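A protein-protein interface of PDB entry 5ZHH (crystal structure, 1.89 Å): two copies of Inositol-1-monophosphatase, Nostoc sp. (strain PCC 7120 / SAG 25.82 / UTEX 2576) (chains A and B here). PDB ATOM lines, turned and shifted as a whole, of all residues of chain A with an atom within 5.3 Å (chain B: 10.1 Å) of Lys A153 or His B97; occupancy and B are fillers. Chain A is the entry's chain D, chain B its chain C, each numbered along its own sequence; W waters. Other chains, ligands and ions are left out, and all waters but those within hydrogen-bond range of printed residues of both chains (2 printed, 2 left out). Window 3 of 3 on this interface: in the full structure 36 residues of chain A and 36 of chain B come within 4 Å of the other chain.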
ATOM      1  N   THR A 148      -5.880 -24.859   3.001  1.00  0.00           N
ATOM      2  CA  THR A 148      -6.097 -23.430   2.767  1.00  0.00           C
ATOM      3  C   THR A 148      -7.408 -23.171   2.033  1.00  0.00           C
ATOM      4  O   THR A 148      -7.699 -23.804   1.015  1.00  0.00           O
ATOM      5  CB  THR A 148      -4.934 -22.862   1.954  1.00  0.00           C
ATOM      6  OG1 THR A 148      -3.696 -23.232   2.571  1.00  0.00           O
ATOM      7  CG2 THR A 148      -5.021 -21.354   1.880  1.00  0.00           C
ATOM      8  N   GLU A 150      -8.706 -19.575   1.881  1.00  0.00           N
ATOM      9  CA  GLU A 150      -8.784 -18.175   1.485  1.00  0.00           C
ATOM     10  C   GLU A 150      -7.740 -17.866   0.422  1.00  0.00           C
ATOM     11  O   GLU A 150      -6.561 -18.191   0.585  1.00  0.00           O
ATOM     12  CB  GLU A 150      -8.576 -17.250   2.684  1.00  0.00           C
ATOM     13  CG  GLU A 150      -9.609 -17.380   3.780  1.00  0.00           C
ATOM     14  CD  GLU A 150      -9.248 -16.548   4.989  1.00  0.00           C
ATOM     15  OE1 GLU A 150      -9.338 -17.065   6.122  1.00  0.00           O
ATOM     16  OE2 GLU A 150      -8.865 -15.374   4.802  1.00  0.00           O
ATOM     17  N   LEU A 151      -8.175 -17.175  -0.635  1.00  0.00           N
ATOM     18  CA  LEU A 151      -7.270 -16.822  -1.723  1.00  0.00           C
ATOM     19  C   LEU A 151      -6.123 -15.955  -1.232  1.00  0.00           C
ATOM     20  O   LEU A 151      -4.981 -16.126  -1.668  1.00  0.00           O
ATOM     21  CB  LEU A 151      -8.041 -16.103  -2.831  1.00  0.00           C
ATOM     22  CG  LEU A 151      -8.871 -16.987  -3.762  1.00  0.00           C
ATOM     23  CD1 LEU A 151      -9.616 -16.119  -4.775  1.00  0.00           C
ATOM     24  CD2 LEU A 151      -8.013 -18.041  -4.453  1.00  0.00           C
ATOM     25  N   SER A 152      -6.402 -15.032  -0.302  1.00  0.00           N
ATOM     26  CA  SER A 152      -5.368 -14.149   0.233  1.00  0.00           C
ATOM     27  C   SER A 152      -4.234 -14.893   0.935  1.00  0.00           C
ATOM     28  O   SER A 152      -3.135 -14.342   1.058  1.00  0.00           O
ATOM     29  CB  SER A 152      -6.000 -13.140   1.194  1.00  0.00           C
ATOM     30  OG  SER A 152      -6.494 -13.782   2.357  1.00  0.00           O
ATOM     31  N   LYS A 153      -4.467 -16.115   1.405  1.00  0.00           N
ATOM     32  CA  LYS A 153      -3.436 -16.901   2.074  1.00  0.00           C
ATOM     33  C   LYS A 153      -2.903 -18.027   1.196  1.00  0.00           C
ATOM     34  O   LYS A 153      -2.134 -18.871   1.676  1.00  0.00           O
ATOM     35  CB  LYS A 153      -3.972 -17.479   3.385  1.00  0.00           C
ATOM     36  CG  LYS A 153      -4.414 -16.439   4.403  1.00  0.00           C
ATOM     37  CD  LYS A 153      -5.185 -17.112   5.522  1.00  0.00           C
ATOM     38  CE  LYS A 153      -5.663 -16.115   6.565  1.00  0.00           C
ATOM     39  NZ  LYS A 153      -6.391 -16.826   7.654  1.00  0.00           N
ATOM     40  N   SER A 154      -3.296 -18.070  -0.074  1.00  0.00           N
ATOM     41  CA  SER A 154      -2.979 -19.199  -0.938  1.00  0.00           C
ATOM     42  C   SER A 154      -1.781 -18.936  -1.845  1.00  0.00           C
ATOM     43  O   SER A 154      -1.402 -17.795  -2.117  1.00  0.00           O
ATOM     44  CB  SER A 154      -4.196 -19.577  -1.784  1.00  0.00           C
ATOM     45  OG  SER A 154      -4.421 -18.634  -2.816  1.00  0.00           O
ATOM     46  N   LEU A 155      -1.156 -20.038  -2.270  1.00  0.00           N
ATOM     47  CA  LEU A 155      -0.121 -20.049  -3.297  1.00  0.00           C
ATOM     48  C   LEU A 155      -0.635 -20.914  -4.439  1.00  0.00           C
ATOM     49  O   LEU A 155      -1.003 -22.076  -4.226  1.00  0.00           O
ATOM     50  CB  LEU A 155       1.202 -20.608  -2.761  1.00  0.00           C
ATOM     51  CG  LEU A 155       2.415 -20.596  -3.702  1.00  0.00           C
ATOM     52  CD1 LEU A 155       2.847 -19.172  -4.034  1.00  0.00           C
ATOM     53  CD2 LEU A 155       3.581 -21.394  -3.112  1.00  0.00           C
ATOM     54  N   GLN A 183      -1.157 -14.931  -2.382  1.00  0.00           N
ATOM     55  CA  GLN A 183       0.230 -14.735  -1.991  1.00  0.00           C
ATOM     56  C   GLN A 183       1.190 -14.893  -3.164  1.00  0.00           C
ATOM     57  O   GLN A 183       2.371 -14.563  -3.021  1.00  0.00           O
ATOM     58  CB  GLN A 183       0.607 -15.714  -0.877  1.00  0.00           C
ATOM     59  CG  GLN A 183      -0.033 -15.382   0.470  1.00  0.00           C
ATOM     60  CD  GLN A 183       0.281 -16.428   1.523  1.00  0.00           C
ATOM     61  OE1 GLN A 183       0.865 -17.465   1.220  1.00  0.00           O
ATOM     62  NE2 GLN A 183      -0.118 -16.166   2.762  1.00  0.00           N
ATOM     63  N   GLY A 201       0.357 -30.606  -1.411  1.00  0.00           N
ATOM     64  CA  GLY A 201       0.135 -29.416  -0.615  1.00  0.00           C
ATOM     65  C   GLY A 201       1.163 -28.320  -0.777  1.00  0.00           C
ATOM     66  O   GLY A 201       1.117 -27.336  -0.027  1.00  0.00           O
ATOM     67  N   ARG A 202       2.082 -28.444  -1.737  1.00  0.00           N
ATOM     68  CA  ARG A 202       3.073 -27.392  -1.937  1.00  0.00           C
ATOM     69  C   ARG A 202       2.446 -26.147  -2.546  1.00  0.00           C
ATOM     70  O   ARG A 202       2.968 -25.042  -2.367  1.00  0.00           O
ATOM     71  CB  ARG A 202       4.205 -27.890  -2.830  1.00  0.00           C
ATOM     72  CG  ARG A 202       5.126 -28.885  -2.137  1.00  0.00           C
ATOM     73  CD  ARG A 202       5.988 -29.617  -3.136  1.00  0.00           C
ATOM     74  NE  ARG A 202       6.829 -30.606  -2.471  1.00  0.00           N
ATOM     75  CZ  ARG A 202       7.741 -31.348  -3.087  1.00  0.00           C
ATOM     76  NH1 ARG A 202       8.455 -32.220  -2.390  1.00  0.00           N
ATOM     77  NH2 ARG A 202       7.932 -31.225  -4.396  1.00  0.00           N
ATOM     78  N   VAL A 203       1.347 -26.307  -3.281  1.00  0.00           N
ATOM     79  CA  VAL A 203       0.490 -25.200  -3.682  1.00  0.00           C
ATOM     80  C   VAL A 203      -0.938 -25.591  -3.328  1.00  0.00           C
ATOM     81  O   VAL A 203      -1.229 -26.748  -3.015  1.00  0.00           O
ATOM     82  CB  VAL A 203       0.610 -24.852  -5.184  1.00  0.00           C
ATOM     83  CG1 VAL A 203       2.019 -24.383  -5.519  1.00  0.00           C
ATOM     84  CG2 VAL A 203       0.218 -26.029  -6.044  1.00  0.00           C
ATOM     85  N   ASP A 204      -1.828 -24.603  -3.351  1.00  0.00           N
ATOM     86  CA  ASP A 204      -3.220 -24.828  -2.991  1.00  0.00           C
ATOM     87  C   ASP A 204      -4.125 -25.031  -4.195  1.00  0.00           C
ATOM     88  O   ASP A 204      -5.249 -25.519  -4.030  1.00  0.00           O
ATOM     89  CB  ASP A 204      -3.736 -23.652  -2.158  1.00  0.00           C
ATOM     90  CG  ASP A 204      -2.853 -23.372  -0.964  1.00  0.00           C
ATOM     91  OD1 ASP A 204      -2.643 -24.304  -0.162  1.00  0.00           O
ATOM     92  OD2 ASP A 204      -2.362 -22.233  -0.835  1.00  0.00           O
ATOM     93  N   LEU B  26      11.773 -27.977   8.889  1.00  0.00           N
ATOM     94  CA  LEU B  26      10.804 -28.501   7.930  1.00  0.00           C
ATOM     95  C   LEU B  26      10.074 -29.714   8.494  1.00  0.00           C
ATOM     96  O   LEU B  26       8.872 -29.887   8.261  1.00  0.00           O
ATOM     97  CB  LEU B  26      11.491 -28.867   6.613  1.00  0.00           C
ATOM     98  CG  LEU B  26      11.783 -27.757   5.604  1.00  0.00           C
ATOM     99  CD1 LEU B  26      12.438 -28.340   4.361  1.00  0.00           C
ATOM    100  CD2 LEU B  26      10.499 -27.047   5.236  1.00  0.00           C
ATOM    101  N   VAL B  43       7.901 -20.913  10.764  1.00  0.00           N
ATOM    102  CA  VAL B  43       8.393 -20.123   9.641  1.00  0.00           C
ATOM    103  C   VAL B  43       9.120 -18.884  10.160  1.00  0.00           C
ATOM    104  O   VAL B  43      10.260 -18.611   9.772  1.00  0.00           O
ATOM    105  CB  VAL B  43       7.255 -19.726   8.680  1.00  0.00           C
ATOM    106  CG1 VAL B  43       7.800 -18.876   7.533  1.00  0.00           C
ATOM    107  CG2 VAL B  43       6.544 -20.965   8.149  1.00  0.00           C
ATOM    108  N   LEU B  89      16.481 -16.528   5.012  1.00  0.00           N
ATOM    109  CA  LEU B  89      15.453 -17.377   4.411  1.00  0.00           C
ATOM    110  C   LEU B  89      14.843 -16.579   3.253  1.00  0.00           C
ATOM    111  O   LEU B  89      13.885 -15.831   3.443  1.00  0.00           O
ATOM    112  CB  LEU B  89      14.398 -17.788   5.420  1.00  0.00           C
ATOM    113  CG  LEU B  89      13.204 -18.628   4.940  1.00  0.00           C
ATOM    114  CD1 LEU B  89      13.634 -19.701   3.972  1.00  0.00           C
ATOM    115  CD2 LEU B  89      12.490 -19.254   6.129  1.00  0.00           C
ATOM    116  N   GLY B  91      12.605 -16.620   0.035  1.00  0.00           N
ATOM    117  CA  GLY B  91      11.520 -17.480  -0.390  1.00  0.00           C
ATOM    118  C   GLY B  91      10.621 -17.851   0.769  1.00  0.00           C
ATOM    119  O   GLY B  91      10.248 -19.013   0.927  1.00  0.00           O
ATOM    120  N   THR B  92      10.255 -16.866   1.590  1.00  0.00           N
ATOM    121  CA  THR B  92       9.506 -17.179   2.805  1.00  0.00           C
ATOM    122  C   THR B  92       8.116 -17.715   2.481  1.00  0.00           C
ATOM    123  O   THR B  92       7.627 -18.623   3.160  1.00  0.00           O
ATOM    124  CB  THR B  92       9.428 -15.961   3.726  1.00  0.00           C
ATOM    125  OG1 THR B  92       9.029 -14.807   2.979  1.00  0.00           O
ATOM    126  CG2 THR B  92      10.784 -15.700   4.358  1.00  0.00           C
ATOM    127  N   THR B  93       7.449 -17.154   1.466  1.00  0.00           N
ATOM    128  CA  THR B  93       6.153 -17.693   1.057  1.00  0.00           C
ATOM    129  C   THR B  93       6.272 -19.154   0.630  1.00  0.00           C
ATOM    130  O   THR B  93       5.472 -20.001   1.044  1.00  0.00           O
ATOM    131  CB  THR B  93       5.553 -16.849  -0.070  1.00  0.00           C
ATOM    132  OG1 THR B  93       5.285 -15.526   0.410  1.00  0.00           O
ATOM    133  CG2 THR B  93       4.245 -17.461  -0.557  1.00  0.00           C
ATOM    134  N   ASN B  94       7.269 -19.465  -0.202  1.00  0.00           N
ATOM    135  CA  ASN B  94       7.515 -20.848  -0.604  1.00  0.00           C
ATOM    136  C   ASN B  94       7.743 -21.739   0.611  1.00  0.00           C
ATOM    137  O   ASN B  94       7.163 -22.826   0.726  1.00  0.00           O
ATOM    138  CB  ASN B  94       8.725 -20.909  -1.539  1.00  0.00           C
ATOM    139  CG  ASN B  94       8.405 -20.402  -2.937  1.00  0.00           C
ATOM    140  OD1 ASN B  94       7.240 -20.190  -3.278  1.00  0.00           O
ATOM    141  ND2 ASN B  94       9.438 -20.225  -3.757  1.00  0.00           N
ATOM    142  N   TYR B  95       8.590 -21.282   1.535  1.00  0.00           N
ATOM    143  CA  TYR B  95       8.918 -22.085   2.707  1.00  0.00           C
ATOM    144  C   TYR B  95       7.674 -22.404   3.524  1.00  0.00           C
ATOM    145  O   TYR B  95       7.459 -23.558   3.916  1.00  0.00           O
ATOM    146  CB  TYR B  95       9.953 -21.343   3.553  1.00  0.00           C
ATOM    147  CG  TYR B  95      10.521 -22.151   4.696  1.00  0.00           C
ATOM    148  CD1 TYR B  95      11.597 -23.008   4.500  1.00  0.00           C
ATOM    149  CD2 TYR B  95       9.994 -22.032   5.978  1.00  0.00           C
ATOM    150  CE1 TYR B  95      12.121 -23.744   5.551  1.00  0.00           C
ATOM    151  CE2 TYR B  95      10.514 -22.760   7.037  1.00  0.00           C
ATOM    152  CZ  TYR B  95      11.572 -23.609   6.821  1.00  0.00           C
ATOM    153  OH  TYR B  95      12.083 -24.335   7.880  1.00  0.00           O
ATOM    154  N   ALA B  96       6.821 -21.397   3.752  1.00  0.00           N
ATOM    155  CA  ALA B  96       5.589 -21.599   4.507  1.00  0.00           C
ATOM    156  C   ALA B  96       4.688 -22.631   3.849  1.00  0.00           C
ATOM    157  O   ALA B  96       3.946 -23.336   4.539  1.00  0.00           O
ATOM    158  CB  ALA B  96       4.847 -20.268   4.669  1.00  0.00           C
ATOM    159  N   HIS B  97       4.728 -22.732   2.524  1.00  0.00           N
ATOM    160  CA  HIS B  97       3.933 -23.708   1.795  1.00  0.00           C
ATOM    161  C   HIS B  97       4.712 -24.975   1.496  1.00  0.00           C
ATOM    162  O   HIS B  97       4.158 -25.903   0.896  1.00  0.00           O
ATOM    163  CB  HIS B  97       3.418 -23.100   0.485  1.00  0.00           C
ATOM    164  CG  HIS B  97       2.353 -22.063   0.675  1.00  0.00           C
ATOM    165  ND1 HIS B  97       1.008 -22.356   0.596  1.00  0.00           N
ATOM    166  CD2 HIS B  97       2.433 -20.741   0.957  1.00  0.00           C
ATOM    167  CE1 HIS B  97       0.306 -21.257   0.806  1.00  0.00           C
ATOM    168  NE2 HIS B  97       1.146 -20.263   1.034  1.00  0.00           N
ATOM    169  N   GLN B  98       5.974 -25.040   1.929  1.00  0.00           N
ATOM    170  CA  GLN B  98       6.911 -26.106   1.567  1.00  0.00           C
ATOM    171  C   GLN B  98       7.087 -26.229   0.058  1.00  0.00           C
ATOM    172  O   GLN B  98       7.392 -27.311  -0.453  1.00  0.00           O
ATOM    173  CB  GLN B  98       6.499 -27.451   2.168  1.00  0.00           C
ATOM    174  CG  GLN B  98       6.446 -27.445   3.682  1.00  0.00           C
ATOM    175  CD  GLN B  98       5.034 -27.323   4.204  1.00  0.00           C
ATOM    176  OE1 GLN B  98       4.481 -26.224   4.291  1.00  0.00           O
ATOM    177  NE2 GLN B  98       4.433 -28.461   4.548  1.00  0.00           N
ATOM    178  N   TYR B  99       6.897 -25.131  -0.655  1.00  0.00           N
ATOM    179  CA  TYR B  99       7.190 -25.078  -2.082  1.00  0.00           C
ATOM    180  C   TYR B  99       8.703 -25.072  -2.256  1.00  0.00           C
ATOM    181  O   TYR B  99       9.379 -24.209  -1.679  1.00  0.00           O
ATOM    182  CB  TYR B  99       6.563 -23.825  -2.712  1.00  0.00           C
ATOM    183  CG  TYR B  99       6.536 -23.861  -4.223  1.00  0.00           C
ATOM    184  CD1 TYR B  99       5.489 -24.466  -4.905  1.00  0.00           C
ATOM    185  CD2 TYR B  99       7.583 -23.333  -4.969  1.00  0.00           C
ATOM    186  CE1 TYR B  99       5.473 -24.515  -6.295  1.00  0.00           C
ATOM    187  CE2 TYR B  99       7.571 -23.375  -6.353  1.00  0.00           C
ATOM    188  CZ  TYR B  99       6.517 -23.968  -7.009  1.00  0.00           C
ATOM    189  OH  TYR B  99       6.510 -24.019  -8.390  1.00  0.00           O
ATOM    190  N   PRO B 100       9.305 -26.049  -3.058  1.00  0.00           N
ATOM    191  CA  PRO B 100      10.769 -26.257  -3.037  1.00  0.00           C
ATOM    192  C   PRO B 100      11.532 -25.201  -3.826  1.00  0.00           C
ATOM    193  O   PRO B 100      12.108 -25.446  -4.891  1.00  0.00           O
ATOM    194  CB  PRO B 100      10.915 -27.665  -3.640  1.00  0.00           C
ATOM    195  CG  PRO B 100       9.530 -28.240  -3.718  1.00  0.00           C
ATOM    196  CD  PRO B 100       8.623 -27.065  -3.869  1.00  0.00           C
ATOM    197  N   ALA B 101      11.522 -23.980  -3.306  1.00  0.00           N
ATOM    198  CA  ALA B 101      12.345 -22.923  -3.872  1.00  0.00           C
ATOM    199  C   ALA B 101      12.630 -21.878  -2.799  1.00  0.00           C
ATOM    200  O   ALA B 101      12.033 -20.795  -2.796  1.00  0.00           O
ATOM    201  CB  ALA B 101      11.667 -22.295  -5.093  1.00  0.00           C
ATOM    202  N   PHE B 102      13.561 -22.194  -1.904  1.00  0.00           N
ATOM    203  CA  PHE B 102      13.983 -21.274  -0.860  1.00  0.00           C
ATOM    204  C   PHE B 102      15.451 -21.532  -0.569  1.00  0.00           C
ATOM    205  O   PHE B 102      15.990 -22.590  -0.902  1.00  0.00           O
ATOM    206  CB  PHE B 102      13.148 -21.430   0.422  1.00  0.00           C
ATOM    207  CG  PHE B 102      13.128 -22.831   0.971  1.00  0.00           C
ATOM    208  CD1 PHE B 102      14.162 -23.290   1.778  1.00  0.00           C
ATOM    209  CD2 PHE B 102      12.067 -23.679   0.702  1.00  0.00           C
ATOM    210  CE1 PHE B 102      14.146 -24.583   2.285  1.00  0.00           C
ATOM    211  CE2 PHE B 102      12.047 -24.968   1.207  1.00  0.00           C
ATOM    212  CZ  PHE B 102      13.089 -25.418   1.997  1.00  0.00           C
ATOM    213  N   PHE B 123      16.943 -27.682   0.502  1.00  0.00           N
ATOM    214  CA  PHE B 123      16.015 -28.748   0.142  1.00  0.00           C
ATOM    215  C   PHE B 123      16.577 -29.599  -0.991  1.00  0.00           C
ATOM    216  O   PHE B 123      16.492 -30.832  -0.955  1.00  0.00           O
ATOM    217  CB  PHE B 123      14.659 -28.154  -0.243  1.00  0.00           C
ATOM    218  CG  PHE B 123      13.571 -29.175  -0.399  1.00  0.00           C
ATOM    219  CD1 PHE B 123      12.851 -29.607   0.703  1.00  0.00           C
ATOM    220  CD2 PHE B 123      13.285 -29.722  -1.639  1.00  0.00           C
ATOM    221  CE1 PHE B 123      11.851 -30.556   0.569  1.00  0.00           C
ATOM    222  CE2 PHE B 123      12.286 -30.670  -1.781  1.00  0.00           C
ATOM    223  CZ  PHE B 123      11.572 -31.089  -0.675  1.00  0.00           C
ATOM    224  N   TYR B 162       5.860  -7.152  -3.080  1.00  0.00           N
ATOM    225  CA  TYR B 162       4.818  -7.092  -2.062  1.00  0.00           C
ATOM    226  C   TYR B 162       3.917  -5.876  -2.241  1.00  0.00           C
ATOM    227  O   TYR B 162       2.757  -5.900  -1.814  1.00  0.00           O
ATOM    228  CB  TYR B 162       5.443  -7.103  -0.665  1.00  0.00           C
ATOM    229  CG  TYR B 162       6.029  -8.449  -0.289  1.00  0.00           C
ATOM    230  CD1 TYR B 162       5.199  -9.542  -0.046  1.00  0.00           C
ATOM    231  CD2 TYR B 162       7.402  -8.632  -0.182  1.00  0.00           C
ATOM    232  CE1 TYR B 162       5.724 -10.781   0.296  1.00  0.00           C
ATOM    233  CE2 TYR B 162       7.936  -9.867   0.162  1.00  0.00           C
ATOM    234  CZ  TYR B 162       7.092 -10.936   0.399  1.00  0.00           C
ATOM    235  OH  TYR B 162       7.615 -12.160   0.739  1.00  0.00           O
ATOM    236  N   ARG B 164       2.709  -4.736  -5.027  1.00  0.00           N
ATOM    237  CA  ARG B 164       2.181  -4.766  -6.393  1.00  0.00           C
ATOM    238  C   ARG B 164       0.749  -4.255  -6.513  1.00  0.00           C
ATOM    239  O   ARG B 164       0.352  -3.818  -7.603  1.00  0.00           O
ATOM    240  CB  ARG B 164       2.261  -6.187  -6.955  1.00  0.00           C
ATOM    241  CG  ARG B 164       1.403  -7.194  -6.223  1.00  0.00           C
ATOM    242  CD  ARG B 164       1.808  -8.606  -6.618  1.00  0.00           C
ATOM    243  NE  ARG B 164       1.048  -9.636  -5.920  1.00  0.00           N
ATOM    244  CZ  ARG B 164       1.410 -10.169  -4.758  1.00  0.00           C
ATOM    245  NH1 ARG B 164       2.516  -9.747  -4.146  1.00  0.00           N
ATOM    246  NH2 ARG B 164       0.664 -11.119  -4.200  1.00  0.00           N
ATOM    247  N   ARG B 165      -0.048  -4.316  -5.444  1.00  0.00           N
ATOM    248  CA  ARG B 165      -1.429  -3.836  -5.518  1.00  0.00           C
ATOM    249  C   ARG B 165      -1.559  -2.328  -5.374  1.00  0.00           C
ATOM    250  O   ARG B 165      -2.644  -1.793  -5.583  1.00  0.00           O
ATOM    251  CB  ARG B 165      -2.278  -4.513  -4.435  1.00  0.00           C
ATOM    252  CG  ARG B 165      -2.260  -6.023  -4.466  1.00  0.00           C
ATOM    253  CD  ARG B 165      -2.870  -6.589  -3.196  1.00  0.00           C
ATOM    254  NE  ARG B 165      -2.917  -8.045  -3.215  1.00  0.00           N
ATOM    255  CZ  ARG B 165      -1.962  -8.848  -2.754  1.00  0.00           C
ATOM    256  NH1 ARG B 165      -0.854  -8.348  -2.223  1.00  0.00           N
ATOM    257  NH2 ARG B 165      -2.127 -10.160  -2.828  1.00  0.00           N
ATOM    258  N   SER B 188       9.536 -18.576  -9.755  1.00  0.00           N
ATOM    259  CA  SER B 188       9.969 -19.544  -8.756  1.00  0.00           C
ATOM    260  C   SER B 188       9.619 -19.120  -7.335  1.00  0.00           C
ATOM    261  O   SER B 188       9.297 -19.972  -6.501  1.00  0.00           O
ATOM    262  CB  SER B 188      11.481 -19.759  -8.860  1.00  0.00           C
ATOM    263  OG  SER B 188      12.170 -18.641  -8.305  1.00  0.00           O
HETATM  264  O   HOH W   1       3.790 -13.384  -1.120  1.00  0.00           O
HETATM  265  O   HOH W   2      -2.463 -12.040   0.000  1.00  0.00           O
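The backbone carbonyl oxygen (O) of Gly A201 sits close to the backbone carbonyl oxygen (O) of His B97, 3.5 Å away.
NE2 of His B97 is in hydrogen-bond range of OE1 of Gln A183 (2.8 Å).
Of the 20 printed residues of chain B, 8 touch a printed residue of chain A.
Hydrophobic or aromatic side chains of chain B that line the printed part of chain A: His B97, Tyr B99, Pro B100 and Phe B123.
Among the printed residues, no Asp or Glu carboxylate lies within 4 Å of a Lys or Arg side-chain nitrogen of the other chain.
Lys A153 touches His B97 (O to CE1, 3.5 Å).
CD2 of Leu A155 touches OD1 of Asn B94, at 3.9 Å.
CE1 of His B97 touches N of Leu A155, 3.6 Å away.
CB of Tyr B99 touches CD2 of Leu A155, at 3.9 Å.
Arg B164 touches Gln A183 (NH2 to C, 3.9 Å).
Arg A202 touches His B97 (CA to O, 3.4 Å).
Arg A202 touches Gln B98.
Tyr B99 touches Arg A202.
Arg A202 touches Pro B100.
OD2 of Asp A204 touches CE1 of His B97, at 3.3 Å.
O of Ala B101 is in hydrogen-bond range of ND2 of Asn B94 (2.8 Å).
The side-chain amide nitrogen (ND2) of Asn B94 sits at hydrogen-bond distance from the backbone carbonyl oxygen (O) of Ser B188 (2.8 Å).
The backbone carbonyl oxygen of Leu A155 sits at hydrogen-bond distance from the backbone NH of Asp A204, at 2.8 Å.
O of Asn B94 is in hydrogen-bond range of N of Tyr B99 (2.7 Å).
The backbone carbonyl oxygen (O) of Lys A153 lies close to the side-chain amide oxygen (OE1) of Gln A183.
The side-chain carboxylate (OD1) of Asp A204 lies within hydrogen-bond range of the side-chain hydroxyl (OG1) of Thr A148, 3.1 Å away.
No residue of chain B comes within 4 Å of Glu A150.
Lys A153 touches just one residue of chain B: His B97.
No residue of chain B comes within 4 Å of Ser A154.
Of chain B, only Asn B94 (3.9 Å), His B97 (3.6 Å) and Tyr B99 (3.9 Å) come within 4 Å of Leu A155.
Printed residues of chain B within 4 Å of Gly A201: His B97 (3.5 Å).
Of the printed residues of chain B, Asp A204 touches His B97.
Of the printed residues of chain A, Asn B94 touches Leu A155 (3.9 Å).
His B97 touches six residues of chain A.
Printed residues of chain A within 4 Å of Pro B100: Arg A202.
The nearest residue of chain B that does not touch Lys A153 is Thr B93 (6.9 Å).
The nearest printed residue of chain A that does not touch Asn B94 is Arg A202 (5.7 Å).
Water W2 bridges the backbone carbonyl oxygen (O) of Ser A152 (2.6 Å) and the guanidinium group (NH2) of Arg B165 (3.4 Å).
Water W1 lies within hydrogen-bond range of the backbone carbonyl oxygen of Gln A183 (2.6 Å) and the side-chain hydroxyl of Thr B93 (3.0 Å).
No position is printed for both chains.
Of the 15 pairs that touch across the chains among the printed residues, none has its exchanged pair printed and touching as well.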
